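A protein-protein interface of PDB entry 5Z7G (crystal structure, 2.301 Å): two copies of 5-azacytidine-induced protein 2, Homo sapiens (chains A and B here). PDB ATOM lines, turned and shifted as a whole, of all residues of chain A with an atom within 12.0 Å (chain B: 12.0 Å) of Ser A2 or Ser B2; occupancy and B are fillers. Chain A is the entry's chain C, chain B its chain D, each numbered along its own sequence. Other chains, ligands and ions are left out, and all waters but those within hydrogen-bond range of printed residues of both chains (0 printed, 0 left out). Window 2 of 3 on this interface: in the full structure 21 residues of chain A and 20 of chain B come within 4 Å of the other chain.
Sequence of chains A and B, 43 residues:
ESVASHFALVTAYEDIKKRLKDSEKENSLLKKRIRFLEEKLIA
Ser B2 touches its own counterpart, Ser A2.
Ser A5 touches His B6, and with the chains exchanged His A6 touches Ser B5.
His A6 touches Leu B9, and with the chains exchanged Leu A9 touches His B6.
Leu A9 touches Val B10, and with the chains exchanged Val A10 touches Leu B9.
No residue of chain B comes within 4 Å of Glu A1.
No residue of chain B comes within 4 Å of Val A3.
No residue of chain B comes within 4 Å of Ala A4.
His A6 touches two residues of chain B.
Of the printed residues of chain B, Leu A9 touches His B6 (3.8 Å), Leu B9 (3.6 Å) and Val B10 (3.6 Å).
Printed residues of chain B within 4 Å of Val A10: Leu B9.
No residue of chain A comes within 4 Å of Glu B1.
Ser B2 touches just one residue of chain A: Ser A2.
No residue of chain A comes within 4 Å of Val B3.
Ala B4 touches none of the printed residues of chain A.
Ala B8 touches none of the printed residues of chain A.
Printed residues of chain A within 4 Å of Leu B9: His A6, Leu A9 and Val A10.
Of the printed residues of chain A, Val B10 touches Leu A9 (3.6 Å).
Thr B11 touches none of the printed residues of chain A.
The nearest residue of chain B that does not touch Ser A2 is His B6 (5.3 Å).
The nearest residue of chain A that does not touch Ser B2 is His A6 (5.6 Å).
Hydrophobic or aromatic side chains of chain B that line the printed part of chain A: His B6, Leu B9 and Val B10.
Along chain B the printed residues that touch a printed residue of chain A span positions 2 to 10.
Hydrophobic or aromatic side chains of chain A within 4 Å of the printed part of chain B: His A6, Leu A9 and Val A10.
Among the printed residues, no Asp or Glu carboxylate lies within 4 Å of a Lys or Arg side-chain nitrogen of the other chain.
NE2 of His A6 lies within hydrogen-bond range of OG of Ser B5.
The side-chain hydroxyl (OG) of Ser A5 is in hydrogen-bond range of a ring nitrogen (NE2) of His B6, at 3.4 Å.
Among the printed residues, pairs that only touch across the chains: Ser A2 with Ser B2, His A6 with Leu B9, Leu A9 with His B6, Leu A9 with Leu B9, Leu A9 with Val B10 and Val A10 with Leu B9.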
ATOM      1  N   GLU A   1      -1.011 -16.980  10.596  1.00  0.00           N
ATOM      2  CA  GLU A   1      -1.941 -15.944  11.026  1.00  0.00           C
ATOM      3  C   GLU A   1      -1.628 -14.620  10.335  1.00  0.00           C
ATOM      4  O   GLU A   1      -1.152 -13.673  10.959  1.00  0.00           O
ATOM      5  CB  GLU A   1      -1.891 -15.781  12.547  1.00  0.00           C
ATOM      6  N   SER A   2      -1.907 -14.562   9.031  1.00  0.00           N
ATOM      7  CA  SER A   2      -1.544 -13.388   8.248  1.00  0.00           C
ATOM      8  C   SER A   2      -2.332 -12.150   8.664  1.00  0.00           C
ATOM      9  O   SER A   2      -1.825 -11.026   8.550  1.00  0.00           O
ATOM     10  CB  SER A   2      -1.751 -13.676   6.761  1.00  0.00           C
ATOM     11  OG  SER A   2      -2.152 -12.504   6.068  1.00  0.00           O
ATOM     12  N   VAL A   3      -3.565 -12.327   9.140  1.00  0.00           N
ATOM     13  CA  VAL A   3      -4.361 -11.171   9.534  1.00  0.00           C
ATOM     14  C   VAL A   3      -3.941 -10.675  10.915  1.00  0.00           C
ATOM     15  O   VAL A   3      -3.981  -9.464  11.180  1.00  0.00           O
ATOM     16  CB  VAL A   3      -5.859 -11.512   9.461  1.00  0.00           C
ATOM     17  CG1 VAL A   3      -6.706 -10.351   9.948  1.00  0.00           C
ATOM     18  CG2 VAL A   3      -6.239 -11.871   8.036  1.00  0.00           C
ATOM     19  N   ALA A   4      -3.499 -11.575  11.800  1.00  0.00           N
ATOM     20  CA  ALA A   4      -2.908 -11.132  13.062  1.00  0.00           C
ATOM     21  C   ALA A   4      -1.650 -10.304  12.819  1.00  0.00           C
ATOM     22  O   ALA A   4      -1.436  -9.267  13.461  1.00  0.00           O
ATOM     23  CB  ALA A   4      -2.577 -12.329  13.944  1.00  0.00           C
ATOM     24  N   SER A   5      -0.797 -10.759  11.904  1.00  0.00           N
ATOM     25  CA  SER A   5       0.396 -10.002  11.559  1.00  0.00           C
ATOM     26  C   SER A   5       0.037  -8.631  11.010  1.00  0.00           C
ATOM     27  O   SER A   5       0.664  -7.626  11.367  1.00  0.00           O
ATOM     28  CB  SER A   5       1.220 -10.789  10.549  1.00  0.00           C
ATOM     29  OG  SER A   5       2.251 -10.001  10.008  1.00  0.00           O
ATOM     30  N   HIS A   6      -0.978  -8.573  10.142  1.00  0.00           N
ATOM     31  CA  HIS A   6      -1.420  -7.286   9.620  1.00  0.00           C
ATOM     32  C   HIS A   6      -1.993  -6.413  10.727  1.00  0.00           C
ATOM     33  O   HIS A   6      -1.686  -5.216  10.808  1.00  0.00           O
ATOM     34  CB  HIS A   6      -2.457  -7.485   8.517  1.00  0.00           C
ATOM     35  CG  HIS A   6      -2.759  -6.234   7.752  1.00  0.00           C
ATOM     36  ND1 HIS A   6      -3.722  -5.333   8.151  1.00  0.00           N
ATOM     37  CD2 HIS A   6      -2.206  -5.720   6.627  1.00  0.00           C
ATOM     38  CE1 HIS A   6      -3.758  -4.323   7.298  1.00  0.00           C
ATOM     39  NE2 HIS A   6      -2.846  -4.532   6.365  1.00  0.00           N
ATOM     40  N   PHE A   7      -2.831  -6.992  11.585  1.00  0.00           N
ATOM     41  CA  PHE A   7      -3.376  -6.228  12.699  1.00  0.00           C
ATOM     42  C   PHE A   7      -2.259  -5.652  13.556  1.00  0.00           C
ATOM     43  O   PHE A   7      -2.226  -4.447  13.818  1.00  0.00           O
ATOM     44  CB  PHE A   7      -4.298  -7.107  13.542  1.00  0.00           C
ATOM     45  CG  PHE A   7      -4.829  -6.420  14.772  1.00  0.00           C
ATOM     46  CD1 PHE A   7      -5.890  -5.524  14.681  1.00  0.00           C
ATOM     47  CD2 PHE A   7      -4.271  -6.668  16.023  1.00  0.00           C
ATOM     48  CE1 PHE A   7      -6.386  -4.888  15.816  1.00  0.00           C
ATOM     49  CE2 PHE A   7      -4.757  -6.038  17.163  1.00  0.00           C
ATOM     50  CZ  PHE A   7      -5.818  -5.148  17.057  1.00  0.00           C
ATOM     51  N   ALA A   8      -1.330  -6.499  14.000  1.00  0.00           N
ATOM     52  CA  ALA A   8      -0.269  -6.022  14.879  1.00  0.00           C
ATOM     53  C   ALA A   8       0.525  -4.905  14.226  1.00  0.00           C
ATOM     54  O   ALA A   8       0.953  -3.967  14.902  1.00  0.00           O
ATOM     55  CB  ALA A   8       0.662  -7.169  15.261  1.00  0.00           C
ATOM     56  N   LEU A   9       0.730  -4.991  12.910  1.00  0.00           N
ATOM     57  CA  LEU A   9       1.469  -3.948  12.204  1.00  0.00           C
ATOM     58  C   LEU A   9       0.653  -2.671  12.088  1.00  0.00           C
ATOM     59  O   LEU A   9       1.199  -1.574  12.213  1.00  0.00           O
ATOM     60  CB  LEU A   9       1.888  -4.432  10.820  1.00  0.00           C
ATOM     61  CG  LEU A   9       2.605  -3.422   9.918  1.00  0.00           C
ATOM     62  CD1 LEU A   9       3.850  -2.853  10.575  1.00  0.00           C
ATOM     63  CD2 LEU A   9       2.966  -4.097   8.607  1.00  0.00           C
ATOM     64  N   VAL A  10      -0.655  -2.787  11.849  1.00  0.00           N
ATOM     65  CA  VAL A  10      -1.500  -1.597  11.806  1.00  0.00           C
ATOM     66  C   VAL A  10      -1.414  -0.844  13.127  1.00  0.00           C
ATOM     67  O   VAL A  10      -1.172   0.368  13.151  1.00  0.00           O
ATOM     68  CB  VAL A  10      -2.956  -1.961  11.461  1.00  0.00           C
ATOM     69  CG1 VAL A  10      -3.866  -0.751  11.684  1.00  0.00           C
ATOM     70  CG2 VAL A  10      -3.069  -2.402  10.018  1.00  0.00           C
ATOM     71  N   THR A  11      -1.586  -1.552  14.247  1.00  0.00           N
ATOM     72  CA  THR A  11      -1.588  -0.864  15.535  1.00  0.00           C
ATOM     73  C   THR A  11      -0.216  -0.293  15.862  1.00  0.00           C
ATOM     74  O   THR A  11      -0.116   0.797  16.434  1.00  0.00           O
ATOM     75  CB  THR A  11      -2.064  -1.793  16.654  1.00  0.00           C
ATOM     76  OG1 THR A  11      -0.963  -2.571  17.132  1.00  0.00           O
ATOM     77  CG2 THR A  11      -3.169  -2.716  16.160  1.00  0.00           C
ATOM     78  N   GLU B   1      -2.868 -10.024  -3.456  1.00  0.00           N
ATOM     79  CA  GLU B   1      -3.248  -8.677  -3.055  1.00  0.00           C
ATOM     80  C   GLU B   1      -3.095  -8.478  -1.554  1.00  0.00           C
ATOM     81  O   GLU B   1      -2.713  -7.398  -1.089  1.00  0.00           O
ATOM     82  CB  GLU B   1      -4.692  -8.366  -3.455  1.00  0.00           C
ATOM     83  CG  GLU B   1      -5.135  -6.968  -3.003  1.00  0.00           C
ATOM     84  CD  GLU B   1      -6.617  -6.707  -3.210  1.00  0.00           C
ATOM     85  OE1 GLU B   1      -7.439  -7.495  -2.688  1.00  0.00           O
ATOM     86  OE2 GLU B   1      -6.953  -5.709  -3.893  1.00  0.00           O
ATOM     87  N   SER B   2      -3.425  -9.520  -0.791  1.00  0.00           N
ATOM     88  CA  SER B   2      -3.185  -9.471   0.644  1.00  0.00           C
ATOM     89  C   SER B   2      -1.704  -9.251   0.949  1.00  0.00           C
ATOM     90  O   SER B   2      -1.364  -8.544   1.907  1.00  0.00           O
ATOM     91  CB  SER B   2      -3.699 -10.759   1.293  1.00  0.00           C
ATOM     92  OG  SER B   2      -3.265 -10.877   2.636  1.00  0.00           O
ATOM     93  N   VAL B   3      -0.814  -9.827   0.133  1.00  0.00           N
ATOM     94  CA  VAL B   3       0.620  -9.614   0.304  1.00  0.00           C
ATOM     95  C   VAL B   3       0.997  -8.185  -0.063  1.00  0.00           C
ATOM     96  O   VAL B   3       1.765  -7.529   0.647  1.00  0.00           O
ATOM     97  CB  VAL B   3       1.412 -10.635  -0.531  1.00  0.00           C
ATOM     98  CG1 VAL B   3       2.905 -10.360  -0.441  1.00  0.00           C
ATOM     99  CG2 VAL B   3       1.084 -12.054  -0.086  1.00  0.00           C
ATOM    100  N   ALA B   4       0.467  -7.681  -1.177  1.00  0.00           N
ATOM    101  CA  ALA B   4       0.758  -6.304  -1.563  1.00  0.00           C
ATOM    102  C   ALA B   4       0.322  -5.325  -0.477  1.00  0.00           C
ATOM    103  O   ALA B   4       1.018  -4.343  -0.206  1.00  0.00           O
ATOM    104  CB  ALA B   4       0.081  -5.974  -2.891  1.00  0.00           C
ATOM    105  N   SER B   5      -0.803  -5.601   0.181  1.00  0.00           N
ATOM    106  CA  SER B   5      -1.271  -4.697   1.226  1.00  0.00           C
ATOM    107  C   SER B   5      -0.302  -4.674   2.395  1.00  0.00           C
ATOM    108  O   SER B   5      -0.035  -3.608   2.972  1.00  0.00           O
ATOM    109  CB  SER B   5      -2.664  -5.109   1.694  1.00  0.00           C
ATOM    110  OG  SER B   5      -2.851  -4.751   3.055  1.00  0.00           O
ATOM    111  N   HIS B   6       0.250  -5.836   2.750  1.00  0.00           N
ATOM    112  CA  HIS B   6       1.208  -5.896   3.850  1.00  0.00           C
ATOM    113  C   HIS B   6       2.531  -5.231   3.477  1.00  0.00           C
ATOM    114  O   HIS B   6       3.123  -4.505   4.287  1.00  0.00           O
ATOM    115  CB  HIS B   6       1.429  -7.341   4.256  1.00  0.00           C
ATOM    116  CG  HIS B   6       2.226  -7.496   5.513  1.00  0.00           C
ATOM    117  ND1 HIS B   6       3.604  -7.574   5.516  1.00  0.00           N
ATOM    118  CD2 HIS B   6       1.837  -7.612   6.804  1.00  0.00           C
ATOM    119  CE1 HIS B   6       4.028  -7.730   6.757  1.00  0.00           C
ATOM    120  NE2 HIS B   6       2.976  -7.758   7.557  1.00  0.00           N
ATOM    121  N   PHE B   7       2.989  -5.440   2.241  1.00  0.00           N
ATOM    122  CA  PHE B   7       4.201  -4.775   1.775  1.00  0.00           C
ATOM    123  C   PHE B   7       4.043  -3.257   1.782  1.00  0.00           C
ATOM    124  O   PHE B   7       4.932  -2.536   2.249  1.00  0.00           O
ATOM    125  CB  PHE B   7       4.566  -5.270   0.375  1.00  0.00           C
ATOM    126  CG  PHE B   7       5.735  -4.550  -0.237  1.00  0.00           C
ATOM    127  CD1 PHE B   7       5.535  -3.509  -1.142  1.00  0.00           C
ATOM    128  CD2 PHE B   7       7.038  -4.912   0.086  1.00  0.00           C
ATOM    129  CE1 PHE B   7       6.619  -2.837  -1.713  1.00  0.00           C
ATOM    130  CE2 PHE B   7       8.125  -4.246  -0.481  1.00  0.00           C
ATOM    131  CZ  PHE B   7       7.916  -3.208  -1.381  1.00  0.00           C
ATOM    132  N   ALA B   8       2.928  -2.749   1.244  1.00  0.00           N
ATOM    133  CA  ALA B   8       2.762  -1.301   1.181  1.00  0.00           C
ATOM    134  C   ALA B   8       2.732  -0.695   2.572  1.00  0.00           C
ATOM    135  O   ALA B   8       3.185   0.436   2.763  1.00  0.00           O
ATOM    136  CB  ALA B   8       1.492  -0.918   0.409  1.00  0.00           C
ATOM    137  N   LEU B   9       2.221  -1.438   3.553  1.00  0.00           N
ATOM    138  CA  LEU B   9       2.151  -0.912   4.909  1.00  0.00           C
ATOM    139  C   LEU B   9       3.521  -0.922   5.574  1.00  0.00           C
ATOM    140  O   LEU B   9       3.871   0.032   6.276  1.00  0.00           O
ATOM    141  CB  LEU B   9       1.136  -1.716   5.721  1.00  0.00           C
ATOM    142  CG  LEU B   9       0.979  -1.432   7.204  1.00  0.00           C
ATOM    143  CD1 LEU B   9       0.628   0.036   7.448  1.00  0.00           C
ATOM    144  CD2 LEU B   9      -0.103  -2.345   7.786  1.00  0.00           C
ATOM    145  N   VAL B  10       4.324  -1.978   5.351  1.00  0.00           N
ATOM    146  CA  VAL B  10       5.703  -1.970   5.852  1.00  0.00           C
ATOM    147  C   VAL B  10       6.488  -0.798   5.258  1.00  0.00           C
ATOM    148  O   VAL B  10       7.196  -0.077   5.968  1.00  0.00           O
ATOM    149  CB  VAL B  10       6.392  -3.312   5.561  1.00  0.00           C
ATOM    150  CG1 VAL B  10       7.839  -3.268   6.041  1.00  0.00           C
ATOM    151  CG2 VAL B  10       5.642  -4.446   6.231  1.00  0.00           C
ATOM    152  N   THR B  11       6.344  -0.568   3.957  1.00  0.00           N
ATOM    153  CA  THR B  11       7.010   0.561   3.316  1.00  0.00           C
ATOM    154  C   THR B  11       6.592   1.897   3.925  1.00  0.00           C
ATOM    155  O   THR B  11       7.430   2.786   4.140  1.00  0.00           O
ATOM    156  CB  THR B  11       6.706   0.526   1.820  1.00  0.00           C
ATOM    157  OG1 THR B  11       7.364  -0.611   1.246  1.00  0.00           O
ATOM    158  CG2 THR B  11       7.121   1.824   1.120  1.00  0.00           C
